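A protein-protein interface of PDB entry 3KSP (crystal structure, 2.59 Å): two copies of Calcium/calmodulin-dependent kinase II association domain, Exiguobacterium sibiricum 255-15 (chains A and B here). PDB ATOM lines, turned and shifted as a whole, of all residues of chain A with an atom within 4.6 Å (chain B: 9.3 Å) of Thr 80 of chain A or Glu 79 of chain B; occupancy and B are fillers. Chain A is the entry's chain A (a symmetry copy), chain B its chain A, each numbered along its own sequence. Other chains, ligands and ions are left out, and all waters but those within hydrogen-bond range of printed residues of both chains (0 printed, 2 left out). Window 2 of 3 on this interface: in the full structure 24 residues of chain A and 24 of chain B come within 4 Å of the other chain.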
ATOM      1  N   PHE A  78      11.494 -10.863  19.155  1.00  0.00           N
ATOM      2  CA  PHE A  78      10.483 -11.416  18.271  1.00  0.00           C
ATOM      3  C   PHE A  78      10.168 -12.831  18.779  1.00  0.00           C
ATOM      4  O   PHE A  78      10.357 -13.111  19.970  1.00  0.00           O
ATOM      5  CB  PHE A  78      10.986 -11.369  16.829  1.00  0.00           C
ATOM      6  CG  PHE A  78      11.286  -9.959  16.353  1.00  0.00           C
ATOM      7  CD1 PHE A  78      10.286  -9.159  15.824  1.00  0.00           C
ATOM      8  CD2 PHE A  78      12.565  -9.420  16.467  1.00  0.00           C
ATOM      9  CE1 PHE A  78      10.551  -7.857  15.412  1.00  0.00           C
ATOM     10  CE2 PHE A  78      12.836  -8.120  16.046  1.00  0.00           C
ATOM     11  CZ  PHE A  78      11.832  -7.341  15.520  1.00  0.00           C
ATOM     12  N   GLU A  79       9.660 -13.724  17.928  1.00  0.00           N
ATOM     13  CA  GLU A  79       9.318 -15.066  18.408  1.00  0.00           C
ATOM     14  C   GLU A  79      10.595 -15.895  18.668  1.00  0.00           C
ATOM     15  O   GLU A  79      10.829 -16.334  19.804  1.00  0.00           O
ATOM     16  CB  GLU A  79       8.339 -15.776  17.454  1.00  0.00           C
ATOM     17  CG  GLU A  79       6.914 -15.183  17.453  1.00  0.00           C
ATOM     18  CD  GLU A  79       6.315 -15.029  18.846  1.00  0.00           C
ATOM     19  OE1 GLU A  79       6.261 -16.020  19.602  1.00  0.00           O
ATOM     20  OE2 GLU A  79       5.889 -13.909  19.177  1.00  0.00           O
ATOM     21  N   THR A  80      11.429 -16.053  17.637  1.00  0.00           N
ATOM     22  CA  THR A  80      12.615 -16.926  17.667  1.00  0.00           C
ATOM     23  C   THR A  80      13.972 -16.185  17.655  1.00  0.00           C
ATOM     24  O   THR A  80      15.041 -16.811  17.752  1.00  0.00           O
ATOM     25  CB  THR A  80      12.447 -17.939  16.488  1.00  0.00           C
ATOM     26  OG1 THR A  80      11.866 -19.135  17.028  1.00  0.00           O
ATOM     27  CG2 THR A  80      13.729 -18.265  15.687  1.00  0.00           C
ATOM     28  N   THR A  81      13.907 -14.852  17.571  1.00  0.00           N
ATOM     29  CA  THR A  81      15.058 -13.996  17.425  1.00  0.00           C
ATOM     30  C   THR A  81      14.885 -12.710  18.252  1.00  0.00           C
ATOM     31  O   THR A  81      13.782 -12.333  18.624  1.00  0.00           O
ATOM     32  CB  THR A  81      15.250 -13.603  15.942  1.00  0.00           C
ATOM     33  OG1 THR A  81      14.056 -12.978  15.475  1.00  0.00           O
ATOM     34  CG2 THR A  81      15.571 -14.824  15.062  1.00  0.00           C
ATOM     35  N   TYR A 109      20.149 -12.408  18.266  1.00  0.00           N
ATOM     36  CA  TYR A 109      20.197 -13.584  19.113  1.00  0.00           C
ATOM     37  C   TYR A 109      19.119 -14.554  18.651  1.00  0.00           C
ATOM     38  O   TYR A 109      18.104 -14.155  18.108  1.00  0.00           O
ATOM     39  CB  TYR A 109      20.067 -13.168  20.584  1.00  0.00           C
ATOM     40  CG  TYR A 109      21.128 -12.153  20.953  1.00  0.00           C
ATOM     41  CD1 TYR A 109      20.974 -10.819  20.610  1.00  0.00           C
ATOM     42  CD2 TYR A 109      22.293 -12.526  21.591  1.00  0.00           C
ATOM     43  CE1 TYR A 109      21.932  -9.875  20.904  1.00  0.00           C
ATOM     44  CE2 TYR A 109      23.284 -11.567  21.895  1.00  0.00           C
ATOM     45  CZ  TYR A 109      23.087 -10.242  21.528  1.00  0.00           C
ATOM     46  OH  TYR A 109      24.029  -9.266  21.781  1.00  0.00           O
ATOM     47  N   HIS A 110      19.389 -15.836  18.822  1.00  0.00           N
ATOM     48  CA  HIS A 110      18.526 -16.916  18.362  1.00  0.00           C
ATOM     49  C   HIS A 110      18.101 -17.734  19.577  1.00  0.00           C
ATOM     50  O   HIS A 110      18.928 -18.260  20.320  1.00  0.00           O
ATOM     51  CB  HIS A 110      19.291 -17.780  17.347  1.00  0.00           C
ATOM     52  CG  HIS A 110      18.480 -18.863  16.708  1.00  0.00           C
ATOM     53  ND1 HIS A 110      17.147 -18.712  16.387  1.00  0.00           N
ATOM     54  CD2 HIS A 110      18.826 -20.109  16.306  1.00  0.00           C
ATOM     55  CE1 HIS A 110      16.698 -19.831  15.842  1.00  0.00           C
ATOM     56  NE2 HIS A 110      17.696 -20.692  15.782  1.00  0.00           N
ATOM     57  N   TRP A 111      16.784 -17.814  19.753  1.00  0.00           N
ATOM     58  CA  TRP A 111      16.125 -18.561  20.824  1.00  0.00           C
ATOM     59  C   TRP A 111      15.696 -19.946  20.322  1.00  0.00           C
ATOM     60  O   TRP A 111      14.771 -20.084  19.530  1.00  0.00           O
ATOM     61  CB  TRP A 111      14.923 -17.741  21.312  1.00  0.00           C
ATOM     62  CG  TRP A 111      13.955 -18.422  22.262  1.00  0.00           C
ATOM     63  CD1 TRP A 111      12.761 -19.002  21.930  1.00  0.00           C
ATOM     64  CD2 TRP A 111      14.062 -18.516  23.699  1.00  0.00           C
ATOM     65  NE1 TRP A 111      12.144 -19.470  23.054  1.00  0.00           N
ATOM     66  CE2 TRP A 111      12.914 -19.187  24.154  1.00  0.00           C
ATOM     67  CE3 TRP A 111      15.022 -18.110  24.633  1.00  0.00           C
ATOM     68  CZ2 TRP A 111      12.696 -19.470  25.514  1.00  0.00           C
ATOM     69  CZ3 TRP A 111      14.817 -18.395  25.986  1.00  0.00           C
ATOM     70  CH2 TRP A 111      13.657 -19.066  26.413  1.00  0.00           C
ATOM     71  N   TRP A 116      18.938 -18.828  24.737  1.00  0.00           N
ATOM     72  CA  TRP A 116      19.386 -17.850  23.740  1.00  0.00           C
ATOM     73  C   TRP A 116      20.823 -18.122  23.373  1.00  0.00           C
ATOM     74  O   TRP A 116      21.603 -18.540  24.201  1.00  0.00           O
ATOM     75  CB  TRP A 116      19.327 -16.401  24.250  1.00  0.00           C
ATOM     76  CG  TRP A 116      17.983 -15.764  24.360  1.00  0.00           C
ATOM     77  CD1 TRP A 116      17.298 -15.517  25.509  1.00  0.00           C
ATOM     78  CD2 TRP A 116      17.177 -15.236  23.293  1.00  0.00           C
ATOM     79  NE1 TRP A 116      16.097 -14.894  25.228  1.00  0.00           N
ATOM     80  CE2 TRP A 116      16.004 -14.702  23.876  1.00  0.00           C
ATOM     81  CE3 TRP A 116      17.328 -15.166  21.906  1.00  0.00           C
ATOM     82  CZ2 TRP A 116      14.987 -14.131  23.122  1.00  0.00           C
ATOM     83  CZ3 TRP A 116      16.314 -14.588  21.161  1.00  0.00           C
ATOM     84  CH2 TRP A 116      15.158 -14.074  21.775  1.00  0.00           C
ATOM     85  N   LYS B   7       6.190 -18.268   2.019  1.00  0.00           N
ATOM     86  CA  LYS B   7       6.901 -17.344   2.887  1.00  0.00           C
ATOM     87  C   LYS B   7       8.276 -16.991   2.301  1.00  0.00           C
ATOM     88  O   LYS B   7       8.640 -15.810   2.279  1.00  0.00           O
ATOM     89  CB  LYS B   7       7.040 -17.925   4.302  1.00  0.00           C
ATOM     90  CG  LYS B   7       7.762 -17.026   5.280  1.00  0.00           C
ATOM     91  CD  LYS B   7       7.296 -17.217   6.728  1.00  0.00           C
ATOM     92  CE  LYS B   7       7.955 -18.408   7.401  1.00  0.00           C
ATOM     93  NZ  LYS B   7       8.408 -18.056   8.767  1.00  0.00           N
ATOM     94  N   HIS B   8       9.029 -17.991   1.821  1.00  0.00           N
ATOM     95  CA  HIS B   8      10.389 -17.738   1.318  1.00  0.00           C
ATOM     96  C   HIS B   8      10.310 -17.028  -0.038  1.00  0.00           C
ATOM     97  O   HIS B   8      11.093 -16.120  -0.296  1.00  0.00           O
ATOM     98  CB  HIS B   8      11.262 -19.006   1.253  1.00  0.00           C
ATOM     99  CG  HIS B   8      11.688 -19.557   2.604  1.00  0.00           C
ATOM    100  ND1 HIS B   8      10.795 -19.924   3.597  1.00  0.00           N
ATOM    101  CD2 HIS B   8      12.917 -19.866   3.093  1.00  0.00           C
ATOM    102  CE1 HIS B   8      11.456 -20.387   4.645  1.00  0.00           C
ATOM    103  NE2 HIS B   8      12.744 -20.378   4.356  1.00  0.00           N
ATOM    104  N   GLU B  76      18.792 -15.867   5.845  1.00  0.00           N
ATOM    105  CA  GLU B  76      18.317 -16.832   6.838  1.00  0.00           C
ATOM    106  C   GLU B  76      16.919 -16.426   7.307  1.00  0.00           C
ATOM    107  O   GLU B  76      16.727 -15.326   7.864  1.00  0.00           O
ATOM    108  CB  GLU B  76      19.247 -16.902   8.047  1.00  0.00           C
ATOM    109  CG  GLU B  76      20.735 -17.183   7.744  1.00  0.00           C
ATOM    110  CD  GLU B  76      21.600 -17.051   9.003  1.00  0.00           C
ATOM    111  OE1 GLU B  76      21.887 -15.908   9.453  1.00  0.00           O
ATOM    112  OE2 GLU B  76      21.968 -18.100   9.568  1.00  0.00           O
ATOM    113  N   VAL B  77      15.953 -17.313   7.086  1.00  0.00           N
ATOM    114  CA  VAL B  77      14.578 -17.070   7.484  1.00  0.00           C
ATOM    115  C   VAL B  77      14.315 -17.769   8.805  1.00  0.00           C
ATOM    116  O   VAL B  77      14.600 -18.939   8.949  1.00  0.00           O
ATOM    117  CB  VAL B  77      13.587 -17.569   6.422  1.00  0.00           C
ATOM    118  CG1 VAL B  77      12.158 -17.282   6.874  1.00  0.00           C
ATOM    119  CG2 VAL B  77      13.899 -16.905   5.065  1.00  0.00           C
ATOM    120  N   PHE B  78      13.792 -17.039   9.779  1.00  0.00           N
ATOM    121  CA  PHE B  78      13.414 -17.607  11.061  1.00  0.00           C
ATOM    122  C   PHE B  78      11.880 -17.684  11.082  1.00  0.00           C
ATOM    123  O   PHE B  78      11.255 -17.756  10.016  1.00  0.00           O
ATOM    124  CB  PHE B  78      14.012 -16.767  12.188  1.00  0.00           C
ATOM    125  CG  PHE B  78      15.529 -16.710  12.143  1.00  0.00           C
ATOM    126  CD1 PHE B  78      16.294 -17.700  12.740  1.00  0.00           C
ATOM    127  CD2 PHE B  78      16.190 -15.684  11.474  1.00  0.00           C
ATOM    128  CE1 PHE B  78      17.683 -17.666  12.678  1.00  0.00           C
ATOM    129  CE2 PHE B  78      17.581 -15.643  11.420  1.00  0.00           C
ATOM    130  CZ  PHE B  78      18.325 -16.631  12.019  1.00  0.00           C
ATOM    131  N   GLU B  79      11.251 -17.709  12.258  1.00  0.00           N
ATOM    132  CA  GLU B  79       9.791 -17.821  12.295  1.00  0.00           C
ATOM    133  C   GLU B  79       9.130 -16.495  11.858  1.00  0.00           C
ATOM    134  O   GLU B  79       8.382 -16.471  10.870  1.00  0.00           O
ATOM    135  CB  GLU B  79       9.293 -18.302  13.671  1.00  0.00           C
ATOM    136  CG  GLU B  79       9.626 -19.776  13.985  1.00  0.00           C
ATOM    137  CD  GLU B  79       9.217 -20.742  12.880  1.00  0.00           C
ATOM    138  OE1 GLU B  79       8.036 -20.748  12.478  1.00  0.00           O
ATOM    139  OE2 GLU B  79      10.085 -21.506  12.422  1.00  0.00           O
ATOM    140  N   THR B  80       9.451 -15.404  12.558  1.00  0.00           N
ATOM    141  CA  THR B  80       8.812 -14.090  12.371  1.00  0.00           C
ATOM    142  C   THR B  80       9.715 -13.008  11.736  1.00  0.00           C
ATOM    143  O   THR B  80       9.264 -11.883  11.462  1.00  0.00           O
ATOM    144  CB  THR B  80       8.233 -13.681  13.765  1.00  0.00           C
ATOM    145  OG1 THR B  80       6.850 -14.069  13.786  1.00  0.00           O
ATOM    146  CG2 THR B  80       8.391 -12.192  14.154  1.00  0.00           C
ATOM    147  N   THR B  81      10.974 -13.378  11.480  1.00  0.00           N
ATOM    148  CA  THR B  81      11.996 -12.480  11.003  1.00  0.00           C
ATOM    149  C   THR B  81      12.894 -13.181   9.968  1.00  0.00           C
ATOM    150  O   THR B  81      12.952 -14.401   9.896  1.00  0.00           O
ATOM    151  CB  THR B  81      12.882 -12.003  12.177  1.00  0.00           C
ATOM    152  OG1 THR B  81      13.434 -13.147  12.828  1.00  0.00           O
ATOM    153  CG2 THR B  81      12.085 -11.166  13.193  1.00  0.00           C
ATOM    154  N   ALA B  82      13.586 -12.389   9.164  1.00  0.00           N
ATOM    155  CA  ALA B  82      14.598 -12.897   8.258  1.00  0.00           C
ATOM    156  C   ALA B  82      15.785 -11.960   8.366  1.00  0.00           C
ATOM    157  O   ALA B  82      15.615 -10.758   8.537  1.00  0.00           O
ATOM    158  CB  ALA B  82      14.083 -12.931   6.831  1.00  0.00           C
ATOM    159  N   LEU B  83      16.984 -12.519   8.285  1.00  0.00           N
ATOM    160  CA  LEU B  83      18.234 -11.753   8.395  1.00  0.00           C
ATOM    161  C   LEU B  83      18.999 -11.931   7.079  1.00  0.00           C
ATOM    162  O   LEU B  83      19.311 -13.075   6.679  1.00  0.00           O
ATOM    163  CB  LEU B  83      19.076 -12.254   9.573  1.00  0.00           C
ATOM    164  CG  LEU B  83      20.382 -11.491   9.853  1.00  0.00           C
ATOM    165  CD1 LEU B  83      20.138 -10.233  10.706  1.00  0.00           C
ATOM    166  CD2 LEU B  83      21.393 -12.414  10.531  1.00  0.00           C
ATOM    167  N   LEU B 108      17.044  -6.720   8.493  1.00  0.00           N
ATOM    168  CA  LEU B 108      16.066  -7.597   9.108  1.00  0.00           C
ATOM    169  C   LEU B 108      14.698  -7.295   8.484  1.00  0.00           C
ATOM    170  O   LEU B 108      14.325  -6.122   8.301  1.00  0.00           O
ATOM    171  CB  LEU B 108      16.014  -7.386  10.612  1.00  0.00           C
ATOM    172  CG  LEU B 108      15.325  -8.506  11.386  1.00  0.00           C
ATOM    173  CD1 LEU B 108      16.297  -9.652  11.600  1.00  0.00           C
ATOM    174  CD2 LEU B 108      14.822  -8.016  12.715  1.00  0.00           C
ATOM    175  N   TYR B 109      13.981  -8.358   8.136  1.00  0.00           N
ATOM    176  CA  TYR B 109      12.616  -8.247   7.667  1.00  0.00           C
ATOM    177  C   TYR B 109      11.698  -8.886   8.700  1.00  0.00           C
ATOM    178  O   TYR B 109      12.093  -9.785   9.420  1.00  0.00           O
ATOM    179  CB  TYR B 109      12.496  -8.863   6.267  1.00  0.00           C
ATOM    180  CG  TYR B 109      13.483  -8.227   5.311  1.00  0.00           C
ATOM    181  CD1 TYR B 109      14.814  -8.611   5.318  1.00  0.00           C
ATOM    182  CD2 TYR B 109      13.104  -7.219   4.448  1.00  0.00           C
ATOM    183  CE1 TYR B 109      15.744  -8.032   4.484  1.00  0.00           C
ATOM    184  CE2 TYR B 109      14.049  -6.615   3.590  1.00  0.00           C
ATOM    185  CZ  TYR B 109      15.374  -7.032   3.635  1.00  0.00           C
ATOM    186  OH  TYR B 109      16.345  -6.464   2.834  1.00  0.00           O
ATOM    187  N   HIS B 110      10.489  -8.362   8.798  1.00  0.00           N
ATOM    188  CA  HIS B 110       9.502  -8.774   9.787  1.00  0.00           C
ATOM    189  C   HIS B 110       8.273  -9.291   9.046  1.00  0.00           C
ATOM    190  O   HIS B 110       7.667  -8.587   8.239  1.00  0.00           O
ATOM    191  CB  HIS B 110       9.152  -7.576  10.684  1.00  0.00           C
ATOM    192  CG  HIS B 110       8.229  -7.891  11.819  1.00  0.00           C
ATOM    193  ND1 HIS B 110       8.270  -9.085  12.510  1.00  0.00           N
ATOM    194  CD2 HIS B 110       7.255  -7.153  12.401  1.00  0.00           C
ATOM    195  CE1 HIS B 110       7.339  -9.079  13.449  1.00  0.00           C
ATOM    196  NE2 HIS B 110       6.711  -7.919  13.403  1.00  0.00           N
ATOM    197  N   TRP B 111       7.938 -10.544   9.343  1.00  0.00           N
ATOM    198  CA  TRP B 111       6.787 -11.258   8.790  1.00  0.00           C
ATOM    199  C   TRP B 111       5.598 -11.178   9.755  1.00  0.00           C
ATOM    200  O   TRP B 111       5.588 -11.794  10.815  1.00  0.00           O
ATOM    201  CB  TRP B 111       7.205 -12.710   8.526  1.00  0.00           C
ATOM    202  CG  TRP B 111       6.106 -13.695   8.167  1.00  0.00           C
ATOM    203  CD1 TRP B 111       5.492 -14.575   9.017  1.00  0.00           C
ATOM    204  CD2 TRP B 111       5.562 -13.955   6.855  1.00  0.00           C
ATOM    205  NE1 TRP B 111       4.590 -15.332   8.328  1.00  0.00           N
ATOM    206  CE2 TRP B 111       4.609 -14.979   7.002  1.00  0.00           C
ATOM    207  CE3 TRP B 111       5.779 -13.411   5.585  1.00  0.00           C
ATOM    208  CZ2 TRP B 111       3.862 -15.474   5.919  1.00  0.00           C
ATOM    209  CZ3 TRP B 111       5.034 -13.892   4.503  1.00  0.00           C
ATOM    210  CH2 TRP B 111       4.090 -14.919   4.679  1.00  0.00           C
ATOM    211  N   ALA B 112       4.609 -10.369   9.388  1.00  0.00           N
ATOM    212  CA  ALA B 112       3.375 -10.184  10.175  1.00  0.00           C
ATOM    213  C   ALA B 112       2.223 -10.113   9.198  1.00  0.00           C
ATOM    214  O   ALA B 112       2.382  -9.622   8.073  1.00  0.00           O
ATOM    215  CB  ALA B 112       3.444  -8.898  11.020  1.00  0.00           C
ATOM    216  N   GLY B 115       2.583 -11.140   5.469  1.00  0.00           N
ATOM    217  CA  GLY B 115       3.358 -10.284   4.570  1.00  0.00           C
ATOM    218  C   GLY B 115       4.684  -9.958   5.210  1.00  0.00           C
ATOM    219  O   GLY B 115       4.806 -10.042   6.430  1.00  0.00           O
ATOM    220  N   TRP B 116       5.680  -9.614   4.389  1.00  0.00           N
ATOM    221  CA  TRP B 116       6.989  -9.175   4.883  1.00  0.00           C
ATOM    222  C   TRP B 116       7.078  -7.670   4.812  1.00  0.00           C
ATOM    223  O   TRP B 116       6.536  -7.062   3.916  1.00  0.00           O
ATOM    224  CB  TRP B 116       8.160  -9.727   4.054  1.00  0.00           C
ATOM    225  CG  TRP B 116       8.510 -11.165   4.229  1.00  0.00           C
ATOM    226  CD1 TRP B 116       8.254 -12.171   3.349  1.00  0.00           C
ATOM    227  CD2 TRP B 116       9.231 -11.763   5.321  1.00  0.00           C
ATOM    228  NE1 TRP B 116       8.742 -13.369   3.833  1.00  0.00           N
ATOM    229  CE2 TRP B 116       9.354 -13.143   5.038  1.00  0.00           C
ATOM    230  CE3 TRP B 116       9.777 -11.270   6.508  1.00  0.00           C
ATOM    231  CZ2 TRP B 116       9.978 -14.032   5.904  1.00  0.00           C
ATOM    232  CZ3 TRP B 116      10.404 -12.159   7.362  1.00  0.00           C
ATOM    233  CH2 TRP B 116      10.502 -13.526   7.052  1.00  0.00           C
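The side-chain amino group of Lys 7 of chain B lies within hydrogen-bond range of the backbone carbonyl oxygen of Phe 78 of chain B, at 3.1 Å.
NZ of Lys 7 of chain B lies within hydrogen-bond range of O of Glu 79 of chain B, at 2.6 Å.
The backbone carbonyl oxygen of Thr 80 of chain B is in hydrogen-bond range of a ring nitrogen (ND1) of His 110 of chain B (3.1 Å).
N of Trp 111 of chain B lies within hydrogen-bond range of O of Thr 80 of chain B (2.8 Å).
ND1 of His 110 of chain A lies within hydrogen-bond range of O of Thr 80 of chain A (3.1 Å).
The backbone NH (N) of Trp 111 of chain A sits at hydrogen-bond distance from the backbone carbonyl oxygen (O) of Thr 80 of chain A, 2.8 Å away.
The side-chain hydroxyl (OG1) of Thr 81 of chain B sits at hydrogen-bond distance from the side-chain hydroxyl (OG1) of Thr 81 of chain A (2.7 Å).
Printed residues of chain A within 4 Å of Glu 79 of chain B: Thr 80 (3.8 Å).
His 110 of chain A touches just one residue of chain B: Phe 78 (3.8 Å).
Of the printed residues of chain B, Phe 78 of chain A touches Thr 80, Thr 81, Leu 108 and His 110.
Of the printed residues of chain B, Glu 79 of chain A touches Thr 80.
Printed residues of chain A within 4 Å of Thr 81 of chain B: Phe 78 (3.5 Å) and Thr 81 (2.7 Å).
Printed residues of chain A within 4 Å of Thr 80 of chain B: Phe 78 and Glu 79.
Ala 112 of chain B touches none of the printed residues of chain A.
The nearest printed residue of chain B that does not touch Thr 80 of chain A is Thr 80 of chain B (5.5 Å).
Among the printed residues, pairs that only touch across the chains: Phe 78 of chain A with Thr 80 of chain B (3.8 Å), Phe 78 of chain A with Thr 81 of chain B (3.5 Å), Phe 78 of chain A with Leu 108 of chain B (3.9 Å), Phe 78 of chain A with His 110 of chain B (3.8 Å), Glu 79 of chain A with Thr 80 of chain B (3.8 Å), Thr 80 of chain A with Phe 78 of chain B (3.8 Å), Thr 80 of chain A with Glu 79 of chain B (3.8 Å), Thr 81 of chain A with Phe 78 of chain B (3.5 Å) and His 110 of chain A with Phe 78 of chain B (3.8 Å).
Phe 78 of chain A touches Thr 81 of chain B, and with the chains exchanged Thr 81 of chain A touches Phe 78 of chain B.
Phe 78 of chain A touches His 110 of chain B, and with the chains exchanged His 110 of chain A touches Phe 78 of chain B.
Glu 79 of chain A touches Thr 80 of chain B, and with the chains exchanged Thr 80 of chain A touches Glu 79 of chain B.
Thr 81 of chain A touches its own counterpart, Thr 81 of chain B.
Positions printed for both chains: 78, 79, 80, 81, 109, 110, 111 and 116.
Of the 10 pairs that touch across the chains among the printed residues, 9 have their exchanged pair printed and touching as well.
Of the 8 printed residues of chain A, 5 touch a printed residue of chain B.
Printed residues of chain A that touch a printed residue of chain B: Phe 78, Glu 79, Thr 80, Thr 81 and His 110.
Hydrophobic or aromatic side chains of chain B within 4 Å of the printed part of chain A: Phe 78, Leu 108 and His 110.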
